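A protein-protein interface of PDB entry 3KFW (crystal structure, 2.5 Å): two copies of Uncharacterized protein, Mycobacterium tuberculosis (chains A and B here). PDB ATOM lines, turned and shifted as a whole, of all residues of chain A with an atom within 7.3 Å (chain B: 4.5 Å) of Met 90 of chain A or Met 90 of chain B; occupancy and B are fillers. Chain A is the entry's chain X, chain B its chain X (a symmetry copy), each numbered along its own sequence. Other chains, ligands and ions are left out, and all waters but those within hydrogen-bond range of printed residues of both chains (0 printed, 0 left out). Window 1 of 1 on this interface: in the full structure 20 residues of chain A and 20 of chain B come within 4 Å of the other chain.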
ATOM      1  N   TRP A  88      12.041 -16.052 -18.770  1.00  0.00           N
ATOM      2  CA  TRP A  88      11.997 -14.664 -18.417  1.00  0.00           C
ATOM      3  C   TRP A  88      13.415 -14.119 -18.202  1.00  0.00           C
ATOM      4  O   TRP A  88      14.272 -14.784 -17.613  1.00  0.00           O
ATOM      5  CB  TRP A  88      11.207 -14.510 -17.096  1.00  0.00           C
ATOM      6  CG  TRP A  88       9.762 -14.881 -17.240  1.00  0.00           C
ATOM      7  CD1 TRP A  88       9.240 -16.155 -17.375  1.00  0.00           C
ATOM      8  CD2 TRP A  88       8.648 -13.989 -17.269  1.00  0.00           C
ATOM      9  NE1 TRP A  88       7.884 -16.098 -17.471  1.00  0.00           N
ATOM     10  CE2 TRP A  88       7.479 -14.793 -17.411  1.00  0.00           C
ATOM     11  CE3 TRP A  88       8.515 -12.610 -17.147  1.00  0.00           C
ATOM     12  CZ2 TRP A  88       6.187 -14.247 -17.483  1.00  0.00           C
ATOM     13  CZ3 TRP A  88       7.243 -12.058 -17.181  1.00  0.00           C
ATOM     14  CH2 TRP A  88       6.076 -12.889 -17.382  1.00  0.00           C
ATOM     15  N   HIS A  89      13.661 -12.905 -18.672  1.00  0.00           N
ATOM     16  CA  HIS A  89      14.830 -12.159 -18.246  1.00  0.00           C
ATOM     17  C   HIS A  89      14.579 -11.627 -16.858  1.00  0.00           C
ATOM     18  O   HIS A  89      13.493 -11.124 -16.584  1.00  0.00           O
ATOM     19  CB  HIS A  89      15.128 -11.004 -19.209  1.00  0.00           C
ATOM     20  CG  HIS A  89      15.764 -11.454 -20.492  1.00  0.00           C
ATOM     21  ND1 HIS A  89      15.636 -10.758 -21.684  1.00  0.00           N
ATOM     22  CD2 HIS A  89      16.520 -12.548 -20.766  1.00  0.00           C
ATOM     23  CE1 HIS A  89      16.316 -11.388 -22.620  1.00  0.00           C
ATOM     24  NE2 HIS A  89      16.860 -12.472 -22.090  1.00  0.00           N
ATOM     25  N   MET A  90      15.584 -11.706 -15.991  1.00  0.00           N
ATOM     26  CA  MET A  90      15.450 -11.215 -14.623  1.00  0.00           C
ATOM     27  C   MET A  90      16.612 -10.356 -14.196  1.00  0.00           C
ATOM     28  O   MET A  90      17.772 -10.736 -14.258  1.00  0.00           O
ATOM     29  CB  MET A  90      15.322 -12.372 -13.665  1.00  0.00           C
ATOM     30  CG  MET A  90      14.586 -11.999 -12.396  1.00  0.00           C
ATOM     31  SD  MET A  90      14.191 -13.614 -11.357  1.00  0.00           S
ATOM     32  CE  MET A  90      15.675 -13.198 -10.189  1.00  0.00           C
ATOM     33  N   LEU A  91      16.301  -9.172 -13.741  1.00  0.00           N
ATOM     34  CA  LEU A  91      17.328  -8.305 -13.309  1.00  0.00           C
ATOM     35  C   LEU A  91      17.070  -7.965 -11.835  1.00  0.00           C
ATOM     36  O   LEU A  91      16.057  -7.405 -11.513  1.00  0.00           O
ATOM     37  CB  LEU A  91      17.355  -7.058 -14.198  1.00  0.00           C
ATOM     38  CG  LEU A  91      17.680  -7.216 -15.689  1.00  0.00           C
ATOM     39  CD1 LEU A  91      17.436  -5.837 -16.408  1.00  0.00           C
ATOM     40  CD2 LEU A  91      19.086  -7.683 -15.918  1.00  0.00           C
ATOM     41  N   ILE A  92      18.018  -8.348 -10.976  1.00  0.00           N
ATOM     42  CA  ILE A  92      18.021  -8.145  -9.539  1.00  0.00           C
ATOM     43  C   ILE A  92      18.958  -6.980  -9.222  1.00  0.00           C
ATOM     44  O   ILE A  92      20.140  -7.059  -9.515  1.00  0.00           O
ATOM     45  CB  ILE A  92      18.621  -9.416  -8.818  1.00  0.00           C
ATOM     46  CG1 ILE A  92      17.918 -10.690  -9.241  1.00  0.00           C
ATOM     47  CG2 ILE A  92      18.563  -9.284  -7.264  1.00  0.00           C
ATOM     48  CD1 ILE A  92      16.471 -10.596  -9.034  1.00  0.00           C
ATOM     49  N   MET A 110      14.649   0.685 -16.618  1.00  0.00           N
ATOM     50  CA  MET A 110      13.792  -0.509 -16.594  1.00  0.00           C
ATOM     51  C   MET A 110      12.492  -0.320 -17.403  1.00  0.00           C
ATOM     52  O   MET A 110      12.125  -1.188 -18.182  1.00  0.00           O
ATOM     53  CB  MET A 110      13.497  -0.923 -15.171  1.00  0.00           C
ATOM     54  CG  MET A 110      14.739  -1.278 -14.379  1.00  0.00           C
ATOM     55  SD  MET A 110      15.669  -2.814 -15.150  1.00  0.00           S
ATOM     56  CE  MET A 110      16.557  -3.449 -13.550  1.00  0.00           C
ATOM     57  N   PHE A 115      10.664  -3.774 -18.749  1.00  0.00           N
ATOM     58  CA  PHE A 115      10.658  -4.639 -17.576  1.00  0.00           C
ATOM     59  C   PHE A 115       9.572  -4.177 -16.613  1.00  0.00           C
ATOM     60  O   PHE A 115       9.277  -2.995 -16.560  1.00  0.00           O
ATOM     61  CB  PHE A 115      12.034  -4.627 -16.897  1.00  0.00           C
ATOM     62  CG  PHE A 115      13.055  -5.482 -17.614  1.00  0.00           C
ATOM     63  CD1 PHE A 115      13.683  -5.024 -18.775  1.00  0.00           C
ATOM     64  CD2 PHE A 115      13.391  -6.724 -17.136  1.00  0.00           C
ATOM     65  CE1 PHE A 115      14.600  -5.803 -19.441  1.00  0.00           C
ATOM     66  CE2 PHE A 115      14.319  -7.507 -17.804  1.00  0.00           C
ATOM     67  CZ  PHE A 115      14.903  -7.057 -18.960  1.00  0.00           C
ATOM     68  N   LEU A 118       8.412  -6.732 -10.169  1.00  0.00           N
ATOM     69  CA  LEU A 118       7.724  -7.727  -9.353  1.00  0.00           C
ATOM     70  C   LEU A 118       7.606  -7.232  -7.935  1.00  0.00           C
ATOM     71  O   LEU A 118       6.675  -7.607  -7.214  1.00  0.00           O
ATOM     72  CB  LEU A 118       8.442  -9.079  -9.363  1.00  0.00           C
ATOM     73  CG  LEU A 118       7.838 -10.230  -8.496  1.00  0.00           C
ATOM     74  CD1 LEU A 118       6.346 -10.610  -8.780  1.00  0.00           C
ATOM     75  CD2 LEU A 118       8.704 -11.479  -8.563  1.00  0.00           C
ATOM     76  N   GLY A 121      13.309  -4.090  -6.301  1.00  0.00           N
ATOM     77  CA  GLY A 121      14.621  -4.562  -6.760  1.00  0.00           C
ATOM     78  C   GLY A 121      14.618  -5.813  -7.663  1.00  0.00           C
ATOM     79  O   GLY A 121      15.687  -6.344  -7.990  1.00  0.00           O
ATOM     80  N   VAL A 122      13.425  -6.301  -8.023  1.00  0.00           N
ATOM     81  CA  VAL A 122      13.261  -7.440  -8.884  1.00  0.00           C
ATOM     82  C   VAL A 122      12.446  -7.041 -10.134  1.00  0.00           C
ATOM     83  O   VAL A 122      11.224  -6.827 -10.056  1.00  0.00           O
ATOM     84  CB  VAL A 122      12.468  -8.571  -8.161  1.00  0.00           C
ATOM     85  CG1 VAL A 122      12.494  -9.801  -8.979  1.00  0.00           C
ATOM     86  CG2 VAL A 122      13.041  -8.870  -6.777  1.00  0.00           C
ATOM     87  N   TRP A 123      13.107  -6.969 -11.284  1.00  0.00           N
ATOM     88  CA  TRP A 123      12.475  -6.594 -12.511  1.00  0.00           C
ATOM     89  C   TRP A 123      12.530  -7.789 -13.447  1.00  0.00           C
ATOM     90  O   TRP A 123      13.519  -8.522 -13.430  1.00  0.00           O
ATOM     91  CB  TRP A 123      13.195  -5.404 -13.118  1.00  0.00           C
ATOM     92  CG  TRP A 123      13.153  -4.158 -12.319  1.00  0.00           C
ATOM     93  CD1 TRP A 123      13.987  -3.820 -11.270  1.00  0.00           C
ATOM     94  CD2 TRP A 123      12.292  -3.041 -12.511  1.00  0.00           C
ATOM     95  NE1 TRP A 123      13.694  -2.567 -10.813  1.00  0.00           N
ATOM     96  CE2 TRP A 123      12.656  -2.060 -11.539  1.00  0.00           C
ATOM     97  CE3 TRP A 123      11.243  -2.764 -13.401  1.00  0.00           C
ATOM     98  CZ2 TRP A 123      11.979  -0.845 -11.401  1.00  0.00           C
ATOM     99  CZ3 TRP A 123      10.578  -1.546 -13.286  1.00  0.00           C
ATOM    100  CH2 TRP A 123      10.939  -0.605 -12.286  1.00  0.00           C
ATOM    101  N   MET A 124      11.471  -8.017 -14.232  1.00  0.00           N
ATOM    102  CA  MET A 124      11.406  -9.204 -15.114  1.00  0.00           C
ATOM    103  C   MET A 124      10.680  -8.880 -16.353  1.00  0.00           C
ATOM    104  O   MET A 124       9.948  -7.908 -16.399  1.00  0.00           O
ATOM    105  CB  MET A 124      10.598 -10.351 -14.519  1.00  0.00           C
ATOM    106  CG  MET A 124      11.158 -10.907 -13.314  1.00  0.00           C
ATOM    107  SD  MET A 124       9.918 -12.119 -12.425  1.00  0.00           S
ATOM    108  CE  MET A 124      10.170 -13.665 -13.598  1.00  0.00           C
ATOM    109  N   ARG A 125      10.858  -9.727 -17.350  1.00  0.00           N
ATOM    110  CA  ARG A 125      10.045  -9.687 -18.559  1.00  0.00           C
ATOM    111  C   ARG A 125      10.319 -10.967 -19.324  1.00  0.00           C
ATOM    112  O   ARG A 125      11.300 -11.635 -19.045  1.00  0.00           O
ATOM    113  CB  ARG A 125      10.335  -8.435 -19.421  1.00  0.00           C
ATOM    114  CG  ARG A 125      11.686  -8.452 -20.102  1.00  0.00           C
ATOM    115  CD  ARG A 125      11.554  -8.129 -21.577  1.00  0.00           C
ATOM    116  NE  ARG A 125      10.383  -7.285 -21.784  1.00  0.00           N
ATOM    117  CZ  ARG A 125       9.313  -7.642 -22.480  1.00  0.00           C
ATOM    118  NH1 ARG A 125       9.264  -8.817 -23.047  1.00  0.00           N
ATOM    119  NH2 ARG A 125       8.300  -6.806 -22.583  1.00  0.00           N
ATOM    120  N   LEU A 131      17.254  -8.461 -24.738  1.00  0.00           N
ATOM    121  CA  LEU A 131      17.914  -7.632 -23.719  1.00  0.00           C
ATOM    122  C   LEU A 131      19.392  -7.357 -24.021  1.00  0.00           C
ATOM    123  O   LEU A 131      20.209  -8.271 -24.118  1.00  0.00           O
ATOM    124  CB  LEU A 131      17.817  -8.276 -22.327  1.00  0.00           C
ATOM    125  CG  LEU A 131      18.759  -7.774 -21.211  1.00  0.00           C
ATOM    126  CD1 LEU A 131      18.191  -6.576 -20.452  1.00  0.00           C
ATOM    127  CD2 LEU A 131      19.143  -8.908 -20.262  1.00  0.00           C
ATOM    128  N   LEU A 133      22.144  -5.158 -21.985  1.00  0.00           N
ATOM    129  CA  LEU A 133      22.360  -4.309 -20.823  1.00  0.00           C
ATOM    130  C   LEU A 133      23.133  -3.040 -21.192  1.00  0.00           C
ATOM    131  O   LEU A 133      24.214  -3.136 -21.757  1.00  0.00           O
ATOM    132  CB  LEU A 133      23.053  -5.103 -19.717  1.00  0.00           C
ATOM    133  CG  LEU A 133      22.022  -5.732 -18.777  1.00  0.00           C
ATOM    134  CD1 LEU A 133      22.593  -6.942 -17.981  1.00  0.00           C
ATOM    135  CD2 LEU A 133      21.447  -4.630 -17.879  1.00  0.00           C
ATOM    136  N   VAL A 141      23.441  -4.926 -11.507  1.00  0.00           N
ATOM    137  CA  VAL A 141      22.298  -5.813 -11.346  1.00  0.00           C
ATOM    138  C   VAL A 141      22.819  -7.231 -11.541  1.00  0.00           C
ATOM    139  O   VAL A 141      23.855  -7.423 -12.166  1.00  0.00           O
ATOM    140  CB  VAL A 141      21.199  -5.536 -12.391  1.00  0.00           C
ATOM    141  CG1 VAL A 141      20.429  -4.273 -12.052  1.00  0.00           C
ATOM    142  CG2 VAL A 141      21.793  -5.453 -13.790  1.00  0.00           C
ATOM    143  N   ARG A 142      22.147  -8.234 -11.014  1.00  0.00           N
ATOM    144  CA  ARG A 142      22.539  -9.604 -11.382  1.00  0.00           C
ATOM    145  C   ARG A 142      21.514 -10.127 -12.379  1.00  0.00           C
ATOM    146  O   ARG A 142      20.320  -9.978 -12.161  1.00  0.00           O
ATOM    147  CB  ARG A 142      22.674 -10.502 -10.159  1.00  0.00           C
ATOM    148  CG  ARG A 142      23.160 -11.881 -10.496  1.00  0.00           C
ATOM    149  CD  ARG A 142      24.217 -12.347  -9.569  1.00  0.00           C
ATOM    150  NE  ARG A 142      24.859 -13.546 -10.110  1.00  0.00           N
ATOM    151  CZ  ARG A 142      26.086 -13.935  -9.788  1.00  0.00           C
ATOM    152  NH1 ARG A 142      26.795 -13.225  -8.919  1.00  0.00           N
ATOM    153  NH2 ARG A 142      26.601 -15.030 -10.320  1.00  0.00           N
ATOM    154  N   MET A 143      21.990 -10.678 -13.494  1.00  0.00           N
ATOM    155  CA  MET A 143      21.132 -11.084 -14.585  1.00  0.00           C
ATOM    156  C   MET A 143      20.907 -12.575 -14.409  1.00  0.00           C
ATOM    157  O   MET A 143      21.854 -13.341 -14.300  1.00  0.00           O
ATOM    158  CB  MET A 143      21.799 -10.772 -15.939  1.00  0.00           C
ATOM    159  CG  MET A 143      20.856 -10.603 -17.185  1.00  0.00           C
ATOM    160  SD  MET A 143      20.050 -12.219 -18.091  1.00  0.00           S
ATOM    161  CE  MET A 143      21.660 -13.274 -18.545  1.00  0.00           C
ATOM    162  N   LEU A 144      19.645 -12.978 -14.354  1.00  0.00           N
ATOM    163  CA  LEU A 144      19.294 -14.392 -14.341  1.00  0.00           C
ATOM    164  C   LEU A 144      18.250 -14.652 -15.403  1.00  0.00           C
ATOM    165  O   LEU A 144      17.630 -13.740 -15.913  1.00  0.00           O
ATOM    166  CB  LEU A 144      18.741 -14.795 -12.968  1.00  0.00           C
ATOM    167  CG  LEU A 144      19.574 -14.627 -11.691  1.00  0.00           C
ATOM    168  CD1 LEU A 144      18.727 -14.933 -10.525  1.00  0.00           C
ATOM    169  CD2 LEU A 144      20.646 -15.630 -11.723  1.00  0.00           C
ATOM    170  N   THR A 145      18.054 -15.913 -15.736  1.00  0.00           N
ATOM    171  CA  THR A 145      16.926 -16.348 -16.556  1.00  0.00           C
ATOM    172  C   THR A 145      16.014 -17.104 -15.593  1.00  0.00           C
ATOM    173  O   THR A 145      16.492 -17.795 -14.699  1.00  0.00           O
ATOM    174  CB  THR A 145      17.424 -17.225 -17.764  1.00  0.00           C
ATOM    175  OG1 THR A 145      18.405 -16.489 -18.511  1.00  0.00           O
ATOM    176  CG2 THR A 145      16.281 -17.618 -18.715  1.00  0.00           C
ATOM    177  N   ALA A 146      14.709 -16.951 -15.728  1.00  0.00           N
ATOM    178  CA  ALA A 146      13.815 -17.718 -14.857  1.00  0.00           C
ATOM    179  C   ALA A 146      12.575 -18.219 -15.538  1.00  0.00           C
ATOM    180  O   ALA A 146      12.189 -17.718 -16.605  1.00  0.00           O
ATOM    181  CB  ALA A 146      13.408 -16.904 -13.616  1.00  0.00           C
ATOM    182  N   ARG A 147      11.922 -19.172 -14.892  1.00  0.00           N
ATOM    183  CA  ARG A 147      10.578 -19.529 -15.309  1.00  0.00           C
ATOM    184  C   ARG A 147       9.519 -19.665 -14.206  1.00  0.00           C
ATOM    185  O   ARG A 147       9.799 -20.110 -13.087  1.00  0.00           O
ATOM    186  CB  ARG A 147      10.584 -20.758 -16.259  1.00  0.00           C
ATOM    187  CG  ARG A 147      11.726 -21.738 -16.029  1.00  0.00           C
ATOM    188  CD  ARG A 147      11.540 -23.014 -16.893  1.00  0.00           C
ATOM    189  NE  ARG A 147      11.834 -22.686 -18.269  1.00  0.00           N
ATOM    190  CZ  ARG A 147      11.050 -22.939 -19.307  1.00  0.00           C
ATOM    191  NH1 ARG A 147      11.443 -22.548 -20.495  1.00  0.00           N
ATOM    192  NH2 ARG A 147       9.906 -23.583 -19.170  1.00  0.00           N
ATOM    193  N   TRP B  88      17.942 -23.354 -10.029  1.00  0.00           N
ATOM    194  CA  TRP B  88      17.837 -22.843  -8.695  1.00  0.00           C
ATOM    195  C   TRP B  88      16.363 -22.693  -8.293  1.00  0.00           C
ATOM    196  O   TRP B  88      15.525 -22.261  -9.089  1.00  0.00           O
ATOM    197  CB  TRP B  88      18.504 -21.449  -8.640  1.00  0.00           C
ATOM    198  CG  TRP B  88      19.983 -21.506  -8.877  1.00  0.00           C
ATOM    199  CD1 TRP B  88      20.624 -21.739 -10.081  1.00  0.00           C
ATOM    200  CD2 TRP B  88      21.013 -21.336  -7.904  1.00  0.00           C
ATOM    201  NE1 TRP B  88      21.973 -21.708  -9.907  1.00  0.00           N
ATOM    202  CE2 TRP B  88      22.256 -21.465  -8.591  1.00  0.00           C
ATOM    203  CE3 TRP B  88      21.015 -21.047  -6.544  1.00  0.00           C
ATOM    204  CZ2 TRP B  88      23.496 -21.361  -7.941  1.00  0.00           C
ATOM    205  CZ3 TRP B  88      22.232 -20.906  -5.893  1.00  0.00           C
ATOM    206  CH2 TRP B  88      23.479 -21.097  -6.601  1.00  0.00           C
ATOM    207  N   HIS B  89      16.049 -23.042  -7.054  1.00  0.00           N
ATOM    208  CA  HIS B  89      14.790 -22.638  -6.458  1.00  0.00           C
ATOM    209  C   HIS B  89      14.883 -21.182  -6.079  1.00  0.00           C
ATOM    210  O   HIS B  89      15.896 -20.759  -5.530  1.00  0.00           O
ATOM    211  CB  HIS B  89      14.468 -23.487  -5.222  1.00  0.00           C
ATOM    212  CG  HIS B  89      13.976 -24.863  -5.562  1.00  0.00           C
ATOM    213  ND1 HIS B  89      14.134 -25.953  -4.720  1.00  0.00           N
ATOM    214  CD2 HIS B  89      13.342 -25.325  -6.671  1.00  0.00           C
ATOM    215  CE1 HIS B  89      13.588 -27.010  -5.284  1.00  0.00           C
ATOM    216  NE2 HIS B  89      13.101 -26.656  -6.463  1.00  0.00           N
ATOM    217  N   MET B  90      13.825 -20.422  -6.340  1.00  0.00           N
ATOM    218  CA  MET B  90      13.808 -19.000  -6.009  1.00  0.00           C
ATOM    219  C   MET B  90      12.545 -18.583  -5.301  1.00  0.00           C
ATOM    220  O   MET B  90      11.432 -18.789  -5.760  1.00  0.00           O
ATOM    221  CB  MET B  90      13.963 -18.172  -7.259  1.00  0.00           C
ATOM    222  CG  MET B  90      14.561 -16.809  -6.985  1.00  0.00           C
ATOM    223  SD  MET B  90      15.015 -15.930  -8.678  1.00  0.00           S
ATOM    224  CE  MET B  90      13.413 -14.857  -8.523  1.00  0.00           C
ATOM    225  N   LEU B  91      12.715 -17.970  -4.160  1.00  0.00           N
ATOM    226  CA  LEU B  91      11.585 -17.535  -3.434  1.00  0.00           C
ATOM    227  C   LEU B  91      11.696 -16.014  -3.254  1.00  0.00           C
ATOM    228  O   LEU B  91      12.628 -15.543  -2.660  1.00  0.00           O
ATOM    229  CB  LEU B  91      11.518 -18.275  -2.095  1.00  0.00           C
ATOM    230  CG  LEU B  91      11.325 -19.797  -2.097  1.00  0.00           C
ATOM    231  CD1 LEU B  91      11.503 -20.331  -0.626  1.00  0.00           C
ATOM    232  CD2 LEU B  91       9.988 -20.200  -2.641  1.00  0.00           C
ATOM    233  N   ILE B  92      10.722 -15.291  -3.811  1.00  0.00           N
ATOM    234  CA  ILE B  92      10.588 -13.846  -3.784  1.00  0.00           C
ATOM    235  C   ILE B  92       9.531 -13.483  -2.743  1.00  0.00           C
ATOM    236  O   ILE B  92       8.387 -13.885  -2.878  1.00  0.00           O
ATOM    237  CB  ILE B  92      10.048 -13.329  -5.176  1.00  0.00           C
ATOM    238  CG1 ILE B  92      10.891 -13.831  -6.330  1.00  0.00           C
ATOM    239  CG2 ILE B  92       9.973 -11.772  -5.227  1.00  0.00           C
ATOM    240  CD1 ILE B  92      12.303 -13.489  -6.149  1.00  0.00           C
ATOM    241  N   TRP B 123      15.501 -15.008  -2.026  1.00  0.00           N
ATOM    242  CA  TRP B 123      16.192 -16.124  -1.458  1.00  0.00           C
ATOM    243  C   TRP B 123      16.315 -17.190  -2.532  1.00  0.00           C
ATOM    244  O   TRP B 123      15.396 -17.344  -3.337  1.00  0.00           O
ATOM    245  CB  TRP B 123      15.420 -16.653  -0.263  1.00  0.00           C
ATOM    246  CG  TRP B 123      15.290 -15.717   0.877  1.00  0.00           C
ATOM    247  CD1 TRP B 123      14.350 -14.713   1.020  1.00  0.00           C
ATOM    248  CD2 TRP B 123      16.061 -15.704   2.073  1.00  0.00           C
ATOM    249  NE1 TRP B 123      14.495 -14.093   2.228  1.00  0.00           N
ATOM    250  CE2 TRP B 123      15.538 -14.663   2.898  1.00  0.00           C
ATOM    251  CE3 TRP B 123      17.148 -16.461   2.536  1.00  0.00           C
ATOM    252  CZ2 TRP B 123      16.092 -14.329   4.136  1.00  0.00           C
ATOM    253  CZ3 TRP B 123      17.692 -16.151   3.779  1.00  0.00           C
ATOM    254  CH2 TRP B 123      17.173 -15.087   4.562  1.00  0.00           C
ATOM    255  N   MET B 124      17.448 -17.901  -2.580  1.00  0.00           N
ATOM    256  CA  MET B 124      17.685 -18.903  -3.644  1.00  0.00           C
ATOM    257  C   MET B 124      18.475 -20.028  -3.117  1.00  0.00           C
ATOM    258  O   MET B 124      19.120 -19.899  -2.092  1.00  0.00           O
ATOM    259  CB  MET B 124      18.542 -18.373  -4.787  1.00  0.00           C
ATOM    260  CG  MET B 124      17.941 -17.293  -5.526  1.00  0.00           C
ATOM    261  SD  MET B 124      19.210 -16.442  -6.736  1.00  0.00           S
ATOM    262  CE  MET B 124      19.187 -17.801  -8.144  1.00  0.00           C
ATOM    263  N   ARG B 142       6.614 -15.678  -4.017  1.00  0.00           N
ATOM    264  CA  ARG B 142       6.374 -16.233  -5.358  1.00  0.00           C
ATOM    265  C   ARG B 142       7.515 -17.189  -5.676  1.00  0.00           C
ATOM    266  O   ARG B 142       8.671 -16.851  -5.461  1.00  0.00           O
ATOM    267  CB  ARG B 142       6.223 -15.136  -6.405  1.00  0.00           C
ATOM    268  CG  ARG B 142       5.888 -15.668  -7.767  1.00  0.00           C
ATOM    269  CD  ARG B 142       4.807 -14.897  -8.422  1.00  0.00           C
ATOM    270  NE  ARG B 142       4.317 -15.625  -9.593  1.00  0.00           N
ATOM    271  CZ  ARG B 142       3.107 -15.458 -10.114  1.00  0.00           C
ATOM    272  NH1 ARG B 142       2.273 -14.580  -9.571  1.00  0.00           N
ATOM    273  NH2 ARG B 142       2.734 -16.155 -11.173  1.00  0.00           N
ATOM    274  N   MET B 143       7.178 -18.396  -6.124  1.00  0.00           N
ATOM    275  CA  MET B 143       8.151 -19.447  -6.327  1.00  0.00           C
ATOM    276  C   MET B 143       8.491 -19.422  -7.806  1.00  0.00           C
ATOM    277  O   MET B 143       7.610 -19.484  -8.651  1.00  0.00           O
ATOM    278  CB  MET B 143       7.567 -20.810  -5.908  1.00  0.00           C
ATOM    279  CG  MET B 143       8.586 -21.941  -5.516  1.00  0.00           C
ATOM    280  SD  MET B 143       9.599 -22.950  -6.944  1.00  0.00           S
ATOM    281  CE  MET B 143       8.129 -23.661  -8.058  1.00  0.00           C
ATOM    282  N   LEU B 144       9.776 -19.303  -8.113  1.00  0.00           N
ATOM    283  CA  LEU B 144      10.248 -19.420  -9.487  1.00  0.00           C
ATOM    284  C   LEU B 144      11.390 -20.409  -9.534  1.00  0.00           C
ATOM    285  O   LEU B 144      11.966 -20.755  -8.522  1.00  0.00           O
ATOM    286  CB  LEU B 144      10.725 -18.059 -10.008  1.00  0.00           C
ATOM    287  CG  LEU B 144       9.784 -16.849 -10.061  1.00  0.00           C
ATOM    288  CD1 LEU B 144      10.561 -15.655 -10.437  1.00  0.00           C
ATOM    289  CD2 LEU B 144       8.810 -17.088 -11.133  1.00  0.00           C
ATOM    290  N   ALA B 146      15.134 -20.680 -11.494  1.00  0.00           N
ATOM    291  CA  ALA B 146      16.022 -19.827 -12.288  1.00  0.00           C
ATOM    292  C   ALA B 146      17.350 -20.449 -12.605  1.00  0.00           C
ATOM    293  O   ALA B 146      17.773 -21.414 -11.950  1.00  0.00           O
ATOM    294  CB  ALA B 146      16.257 -18.470 -11.600  1.00  0.00           C
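The side-chain sulfur (SD) of Met 90 of chain B lies close to the side-chain sulfur (SD) of Met 90 of chain A, 3.6 Å away.
Hydrophobic or aromatic side chains of chain A that line the printed part of chain B: Met 90, Leu 118, Met 124, Leu 144 and Ala 146.
Of the 11 printed residues of chain B, 5 touch a printed residue of chain A.
Hydrophobic or aromatic side chains of chain B within 4 Å of the printed part of chain A: Met 90, Ile 92, Met 124, Leu 144 and Ala 146.
Among the printed residues, 7 pairs touch across the chains.
Among the printed residues, no Asp or Glu carboxylate lies within 4 Å of a Lys or Arg side-chain nitrogen of the other chain.
Met 90 of chain B touches its own counterpart, Met 90 of chain A.
Met 124 of chain A touches Leu 144 of chain B, and with the chains exchanged Leu 144 of chain A touches Met 124 of chain B.
Ala 146 of chain A touches its own counterpart, Ala 146 of chain B.
Among the printed residues, merely in contact across the chains: Leu 118 of chain A with Ile 92 of chain B (3.6 Å), Met 124 of chain A with Leu 144 of chain B (3.8 Å), Leu 144 of chain A with Met 124 of chain B (3.8 Å), Thr 145 of chain A with Ala 146 of chain B (3.2 Å), Ala 146 of chain A with Ala 146 of chain B (3.8 Å) and Arg 147 of chain A with Leu 144 of chain B (3.7 Å).
The backbone carbonyl oxygen (O) of Ile 92 of chain B lies within hydrogen-bond range of the backbone NH (N) of Arg 142 of chain B (2.8 Å).
The backbone carbonyl oxygen (O) of Leu 144 of chain A lies within hydrogen-bond range of the backbone NH (N) of Met 90 of chain A.
The backbone carbonyl oxygen of Leu 144 of chain B lies within hydrogen-bond range of the backbone NH of Met 90 of chain B (2.9 Å).
The backbone NH (N) of Trp 88 of chain A is in hydrogen-bond range of the backbone carbonyl oxygen (O) of Ala 146 of chain A.
The backbone carbonyl oxygen (O) of Ala 146 of chain B is in hydrogen-bond range of the backbone NH (N) of Trp 88 of chain B (2.7 Å).
Met 90 of chain A touches just one residue of chain B: Met 90.
Printed residues of chain B within 4 Å of Leu 118 of chain A: Ile 92.
Of the printed residues of chain B, Thr 145 of chain A touches Ala 146.
Printed residues of chain B within 4 Å of Arg 147 of chain A: Leu 144.
Of the printed residues of chain A, Met 90 of chain B touches Met 90.
Of the printed residues of chain A, Ile 92 of chain B touches Leu 118 (3.6 Å).
Printed residues of chain A within 4 Å of Ala 146 of chain B: Thr 145 (3.2 Å) and Ala 146 (3.8 Å).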
